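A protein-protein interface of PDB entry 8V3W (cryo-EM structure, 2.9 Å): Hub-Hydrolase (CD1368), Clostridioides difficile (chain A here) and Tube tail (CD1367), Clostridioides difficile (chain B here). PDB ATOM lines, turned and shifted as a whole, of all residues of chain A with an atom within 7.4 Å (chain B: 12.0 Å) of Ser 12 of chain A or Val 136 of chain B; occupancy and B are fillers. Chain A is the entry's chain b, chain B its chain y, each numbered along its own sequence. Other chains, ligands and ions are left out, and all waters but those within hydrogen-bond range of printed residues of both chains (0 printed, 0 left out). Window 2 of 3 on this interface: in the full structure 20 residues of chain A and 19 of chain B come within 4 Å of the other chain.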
ATOM      1  N   TRP A   5     -17.244  13.677  29.521  1.00  0.00           N
ATOM      2  CA  TRP A   5     -17.571  13.132  28.211  1.00  0.00           C
ATOM      3  C   TRP A   5     -18.081  14.250  27.316  1.00  0.00           C
ATOM      4  O   TRP A   5     -18.759  15.167  27.784  1.00  0.00           O
ATOM      5  CB  TRP A   5     -18.630  12.034  28.308  1.00  0.00           C
ATOM      6  CG  TRP A   5     -18.173  10.806  29.012  1.00  0.00           C
ATOM      7  CD1 TRP A   5     -17.950  10.667  30.345  1.00  0.00           C
ATOM      8  CD2 TRP A   5     -17.891   9.534  28.423  1.00  0.00           C
ATOM      9  NE1 TRP A   5     -17.540   9.390  30.626  1.00  0.00           N
ATOM     10  CE2 TRP A   5     -17.496   8.674  29.461  1.00  0.00           C
ATOM     11  CE3 TRP A   5     -17.929   9.041  27.118  1.00  0.00           C
ATOM     12  CZ2 TRP A   5     -17.143   7.350  29.237  1.00  0.00           C
ATOM     13  CZ3 TRP A   5     -17.580   7.727  26.898  1.00  0.00           C
ATOM     14  CH2 TRP A   5     -17.193   6.896  27.952  1.00  0.00           C
ATOM     15  N   VAL A   6     -17.761  14.172  26.029  1.00  0.00           N
ATOM     16  CA  VAL A   6     -18.129  15.201  25.066  1.00  0.00           C
ATOM     17  C   VAL A   6     -18.838  14.545  23.890  1.00  0.00           C
ATOM     18  O   VAL A   6     -18.350  13.552  23.343  1.00  0.00           O
ATOM     19  CB  VAL A   6     -16.899  15.995  24.590  1.00  0.00           C
ATOM     20  CG1 VAL A   6     -17.265  16.897  23.447  1.00  0.00           C
ATOM     21  CG2 VAL A   6     -16.336  16.812  25.731  1.00  0.00           C
ATOM     22  N   HIS A   7     -19.983  15.100  23.506  1.00  0.00           N
ATOM     23  CA  HIS A   7     -20.761  14.633  22.365  1.00  0.00           C
ATOM     24  C   HIS A   7     -20.587  15.613  21.213  1.00  0.00           C
ATOM     25  O   HIS A   7     -20.844  16.808  21.373  1.00  0.00           O
ATOM     26  CB  HIS A   7     -22.239  14.503  22.729  1.00  0.00           C
ATOM     27  CG  HIS A   7     -22.538  13.388  23.681  1.00  0.00           C
ATOM     28  ND1 HIS A   7     -21.912  13.260  24.902  1.00  0.00           N
ATOM     29  CD2 HIS A   7     -23.404  12.352  23.594  1.00  0.00           C
ATOM     30  CE1 HIS A   7     -22.377  12.192  25.524  1.00  0.00           C
ATOM     31  NE2 HIS A   7     -23.285  11.624  24.752  1.00  0.00           N
ATOM     32  N   ILE A   8     -20.165  15.108  20.056  1.00  0.00           N
ATOM     33  CA  ILE A   8     -19.915  15.933  18.882  1.00  0.00           C
ATOM     34  C   ILE A   8     -21.088  15.795  17.922  1.00  0.00           C
ATOM     35  O   ILE A   8     -21.865  14.839  17.977  1.00  0.00           O
ATOM     36  CB  ILE A   8     -18.579  15.564  18.196  1.00  0.00           C
ATOM     37  CG1 ILE A   8     -17.479  15.385  19.234  1.00  0.00           C
ATOM     38  CG2 ILE A   8     -18.147  16.640  17.223  1.00  0.00           C
ATOM     39  CD1 ILE A   8     -17.054  16.658  19.883  1.00  0.00           C
ATOM     40  N   LYS A   9     -21.212  16.767  17.014  1.00  0.00           N
ATOM     41  CA  LYS A   9     -22.407  16.876  16.181  1.00  0.00           C
ATOM     42  C   LYS A   9     -22.601  15.658  15.288  1.00  0.00           C
ATOM     43  O   LYS A   9     -23.734  15.201  15.096  1.00  0.00           O
ATOM     44  CB  LYS A   9     -22.344  18.147  15.337  1.00  0.00           C
ATOM     45  CG  LYS A   9     -23.566  18.332  14.461  1.00  0.00           C
ATOM     46  CD  LYS A   9     -24.804  18.605  15.297  1.00  0.00           C
ATOM     47  CE  LYS A   9     -26.035  18.738  14.417  1.00  0.00           C
ATOM     48  NZ  LYS A   9     -27.142  19.468  15.090  1.00  0.00           N
ATOM     49  N   ASN A  10     -21.519  15.119  14.725  1.00  0.00           N
ATOM     50  CA  ASN A  10     -21.680  14.013  13.789  1.00  0.00           C
ATOM     51  C   ASN A  10     -22.243  12.760  14.438  1.00  0.00           C
ATOM     52  O   ASN A  10     -22.872  11.956  13.744  1.00  0.00           O
ATOM     53  CB  ASN A  10     -20.349  13.625  13.156  1.00  0.00           C
ATOM     54  CG  ASN A  10     -19.311  13.224  14.186  1.00  0.00           C
ATOM     55  OD1 ASN A  10     -19.600  13.099  15.375  1.00  0.00           O
ATOM     56  ND2 ASN A  10     -18.103  12.958  13.722  1.00  0.00           N
ATOM     57  N   GLY A  11     -22.033  12.576  15.737  1.00  0.00           N
ATOM     58  CA  GLY A  11     -22.410  11.353  16.417  1.00  0.00           C
ATOM     59  C   GLY A  11     -21.298  10.684  17.201  1.00  0.00           C
ATOM     60  O   GLY A  11     -21.546   9.632  17.808  1.00  0.00           O
ATOM     61  N   SER A  12     -20.086  11.227  17.236  1.00  0.00           N
ATOM     62  CA  SER A  12     -18.998  10.622  17.987  1.00  0.00           C
ATOM     63  C   SER A  12     -19.035  11.062  19.445  1.00  0.00           C
ATOM     64  O   SER A  12     -19.465  12.170  19.770  1.00  0.00           O
ATOM     65  CB  SER A  12     -17.650  10.990  17.372  1.00  0.00           C
ATOM     66  OG  SER A  12     -17.534  12.391  17.227  1.00  0.00           O
ATOM     67  N   ILE A  13     -18.579  10.174  20.326  1.00  0.00           N
ATOM     68  CA  ILE A  13     -18.518  10.427  21.761  1.00  0.00           C
ATOM     69  C   ILE A  13     -17.114  10.105  22.249  1.00  0.00           C
ATOM     70  O   ILE A  13     -16.598   9.014  21.985  1.00  0.00           O
ATOM     71  CB  ILE A  13     -19.556   9.593  22.532  1.00  0.00           C
ATOM     72  CG1 ILE A  13     -20.947   9.770  21.925  1.00  0.00           C
ATOM     73  CG2 ILE A  13     -19.557   9.975  23.995  1.00  0.00           C
ATOM     74  CD1 ILE A  13     -22.049   9.186  22.761  1.00  0.00           C
ATOM     75  N   TYR A  14     -16.506  11.037  22.976  1.00  0.00           N
ATOM     76  CA  TYR A  14     -15.139  10.893  23.452  1.00  0.00           C
ATOM     77  C   TYR A  14     -15.086  10.998  24.967  1.00  0.00           C
ATOM     78  O   TYR A  14     -15.838  11.766  25.573  1.00  0.00           O
ATOM     79  CB  TYR A  14     -14.226  11.954  22.846  1.00  0.00           C
ATOM     80  CG  TYR A  14     -14.078  11.863  21.353  1.00  0.00           C
ATOM     81  CD1 TYR A  14     -13.161  10.997  20.781  1.00  0.00           C
ATOM     82  CD2 TYR A  14     -14.845  12.653  20.515  1.00  0.00           C
ATOM     83  CE1 TYR A  14     -13.021  10.915  19.422  1.00  0.00           C
ATOM     84  CE2 TYR A  14     -14.712  12.575  19.154  1.00  0.00           C
ATOM     85  CZ  TYR A  14     -13.798  11.705  18.611  1.00  0.00           C
ATOM     86  OH  TYR A  14     -13.662  11.628  17.246  1.00  0.00           O
ATOM     87  N   ASP A  15     -14.187  10.227  25.569  1.00  0.00           N
ATOM     88  CA  ASP A  15     -13.855  10.335  26.985  1.00  0.00           C
ATOM     89  C   ASP A  15     -12.518  11.060  27.085  1.00  0.00           C
ATOM     90  O   ASP A  15     -11.488  10.534  26.659  1.00  0.00           O
ATOM     91  CB  ASP A  15     -13.790   8.952  27.629  1.00  0.00           C
ATOM     92  CG  ASP A  15     -13.443   9.004  29.101  1.00  0.00           C
ATOM     93  OD1 ASP A  15     -13.553  10.083  29.713  1.00  0.00           O
ATOM     94  OD2 ASP A  15     -13.054   7.958  29.654  1.00  0.00           O
ATOM     95  N   ILE A  52      -7.957  15.826  19.507  1.00  0.00           N
ATOM     96  CA  ILE A  52      -9.194  16.032  18.770  1.00  0.00           C
ATOM     97  C   ILE A  52      -9.684  17.459  18.968  1.00  0.00           C
ATOM     98  O   ILE A  52      -9.314  18.150  19.923  1.00  0.00           O
ATOM     99  CB  ILE A  52     -10.251  15.019  19.229  1.00  0.00           C
ATOM    100  CG1 ILE A  52     -10.350  15.048  20.756  1.00  0.00           C
ATOM    101  CG2 ILE A  52      -9.904  13.630  18.741  1.00  0.00           C
ATOM    102  CD1 ILE A  52     -11.276  14.026  21.330  1.00  0.00           C
ATOM    103  N   ASP A  53     -10.544  17.907  18.058  1.00  0.00           N
ATOM    104  CA  ASP A  53     -11.144  19.225  18.186  1.00  0.00           C
ATOM    105  C   ASP A  53     -12.576  19.106  18.691  1.00  0.00           C
ATOM    106  O   ASP A  53     -13.305  18.180  18.329  1.00  0.00           O
ATOM    107  CB  ASP A  53     -11.092  20.006  16.867  1.00  0.00           C
ATOM    108  CG  ASP A  53     -12.222  19.663  15.922  1.00  0.00           C
ATOM    109  OD1 ASP A  53     -12.602  18.480  15.830  1.00  0.00           O
ATOM    110  OD2 ASP A  53     -12.742  20.592  15.270  1.00  0.00           O
ATOM    111  N   LYS B 132      -1.725   9.365  25.931  1.00  0.00           N
ATOM    112  CA  LYS B 132      -2.611   8.632  25.039  1.00  0.00           C
ATOM    113  C   LYS B 132      -3.690   9.547  24.474  1.00  0.00           C
ATOM    114  O   LYS B 132      -4.228  10.406  25.176  1.00  0.00           O
ATOM    115  CB  LYS B 132      -3.265   7.473  25.788  1.00  0.00           C
ATOM    116  CG  LYS B 132      -2.415   6.224  25.882  1.00  0.00           C
ATOM    117  CD  LYS B 132      -3.234   4.991  25.547  1.00  0.00           C
ATOM    118  CE  LYS B 132      -2.394   3.729  25.619  1.00  0.00           C
ATOM    119  NZ  LYS B 132      -3.093   2.634  26.348  1.00  0.00           N
ATOM    120  N   ILE B 133      -4.014   9.351  23.201  1.00  0.00           N
ATOM    121  CA  ILE B 133      -5.068  10.118  22.541  1.00  0.00           C
ATOM    122  C   ILE B 133      -6.393   9.377  22.700  1.00  0.00           C
ATOM    123  O   ILE B 133      -6.446   8.155  22.502  1.00  0.00           O
ATOM    124  CB  ILE B 133      -4.725  10.373  21.064  1.00  0.00           C
ATOM    125  CG1 ILE B 133      -5.847  11.147  20.372  1.00  0.00           C
ATOM    126  CG2 ILE B 133      -4.426   9.071  20.342  1.00  0.00           C
ATOM    127  CD1 ILE B 133      -5.611  11.371  18.901  1.00  0.00           C
ATOM    128  N   PRO B 134      -7.473  10.059  23.080  1.00  0.00           N
ATOM    129  CA  PRO B 134      -8.745   9.361  23.294  1.00  0.00           C
ATOM    130  C   PRO B 134      -9.293   8.752  22.011  1.00  0.00           C
ATOM    131  O   PRO B 134      -9.051   9.241  20.906  1.00  0.00           O
ATOM    132  CB  PRO B 134      -9.669  10.462  23.827  1.00  0.00           C
ATOM    133  CG  PRO B 134      -9.027  11.739  23.415  1.00  0.00           C
ATOM    134  CD  PRO B 134      -7.560  11.483  23.433  1.00  0.00           C
ATOM    135  N   LYS B 135     -10.038   7.664  22.173  1.00  0.00           N
ATOM    136  CA  LYS B 135     -10.669   6.963  21.065  1.00  0.00           C
ATOM    137  C   LYS B 135     -12.182   7.069  21.183  1.00  0.00           C
ATOM    138  O   LYS B 135     -12.735   6.989  22.283  1.00  0.00           O
ATOM    139  CB  LYS B 135     -10.257   5.489  21.037  1.00  0.00           C
ATOM    140  CG  LYS B 135      -8.823   5.248  20.606  1.00  0.00           C
ATOM    141  CD  LYS B 135      -8.760   4.695  19.191  1.00  0.00           C
ATOM    142  CE  LYS B 135      -7.672   5.375  18.376  1.00  0.00           C
ATOM    143  NZ  LYS B 135      -6.348   5.337  19.061  1.00  0.00           N
ATOM    144  N   VAL B 136     -12.846   7.253  20.043  1.00  0.00           N
ATOM    145  CA  VAL B 136     -14.301   7.323  20.030  1.00  0.00           C
ATOM    146  C   VAL B 136     -14.871   5.949  20.346  1.00  0.00           C
ATOM    147  O   VAL B 136     -14.438   4.934  19.787  1.00  0.00           O
ATOM    148  CB  VAL B 136     -14.806   7.848  18.677  1.00  0.00           C
ATOM    149  CG1 VAL B 136     -14.114   7.134  17.527  1.00  0.00           C
ATOM    150  CG2 VAL B 136     -16.311   7.684  18.572  1.00  0.00           C
ATOM    151  N   THR B 137     -15.833   5.908  21.262  1.00  0.00           N
ATOM    152  CA  THR B 137     -16.450   4.643  21.630  1.00  0.00           C
ATOM    153  C   THR B 137     -17.236   4.078  20.450  1.00  0.00           C
ATOM    154  O   THR B 137     -17.877   4.833  19.712  1.00  0.00           O
ATOM    155  CB  THR B 137     -17.381   4.823  22.826  1.00  0.00           C
ATOM    156  OG1 THR B 137     -18.313   5.876  22.549  1.00  0.00           O
ATOM    157  CG2 THR B 137     -16.588   5.163  24.079  1.00  0.00           C
ATOM    158  N   PRO B 138     -17.200   2.754  20.238  1.00  0.00           N
ATOM    159  CA  PRO B 138     -18.008   2.100  19.206  1.00  0.00           C
ATOM    160  C   PRO B 138     -19.500   2.232  19.483  1.00  0.00           C
ATOM    161  O   PRO B 138     -19.881   2.281  20.653  1.00  0.00           O
ATOM    162  CB  PRO B 138     -17.564   0.636  19.293  1.00  0.00           C
ATOM    163  CG  PRO B 138     -16.202   0.698  19.894  1.00  0.00           C
ATOM    164  CD  PRO B 138     -16.313   1.792  20.911  1.00  0.00           C
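OD1 of Asn 10 of chain A sits at hydrogen-bond distance from N of Ser 12 of chain A, 2.7 Å away. The backbone NH (N) of Val 6 of chain A sits at hydrogen-bond distance from the backbone carbonyl oxygen (O) of Tyr 14 of chain A.
Ser 12 of chain A touches just one residue of chain B: Val 136. Val 136 of chain B touches just these residues of chain A: Ser 12, Ile 13 and Tyr 14. No residue of chain B comes within 4 Å of His 7 of chain A. No residue of chain B comes within 4 Å of Ile 8 of chain A. No residue of chain B comes within 4 Å of Gly 11 of chain A. Of chain B, only Val 136 and Thr 137 come within 4 Å of Ile 13 of chain A. Tyr 14 of chain A touches just one residue of chain B: Val 136 (3.6 Å). Of the printed residues of chain B, Ile 52 of chain A touches Pro 134 (3.8 Å). Printed residues of chain A within 4 Å of Thr 137 of chain B: Trp 5 and Ile 13. Lys 9 of chain A touches none of the printed residues of chain B. The nearest printed residue of chain B that does not touch Ile 52 of chain A is Ile 133 of chain B (4.9 Å).
Printed residues of chain B that touch a printed residue of chain A: Pro 134, Val 136 and Thr 137. Hydrophobic or aromatic side chains of chain B within 4 Å of the printed part of chain A: Pro 134 and Val 136. Of the 13 printed residues of chain A, 6 touch a printed residue of chain B. Printed residues of chain A that touch a printed residue of chain B: Trp 5, Ser 12, Ile 13, Tyr 14, Asp 15 and Ile 52. Hydrophobic or aromatic side chains of chain A within 4 Å of the printed part of chain B: Trp 5, Ile 13, Tyr 14 and Ile 52. Among the printed residues, no Asp or Glu carboxylate lies within 4 Å of a Lys or Arg side-chain nitrogen of the other chain.
The backbone NH of Thr 137 of chain B lies within hydrogen-bond range of the backbone carbonyl oxygen of Ile 13 of chain A.
Trp 5 of chain A touches Thr 137 of chain B (CZ3 to CG2, 3.9 Å). Ser 12 of chain A touches Val 136 of chain B (CB to CG2, 3.8 Å). O of Ile 13 of chain A touches CA of Val 136 of chain B, at 3.5 Å. Tyr 14 of chain A touches Val 136 of chain B (CE1 to CB, 3.6 Å). CB of Pro 134 of chain B touches O of Asp 15 of chain A, at 3.4 Å. Ile 52 of chain A touches Pro 134 of chain B.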
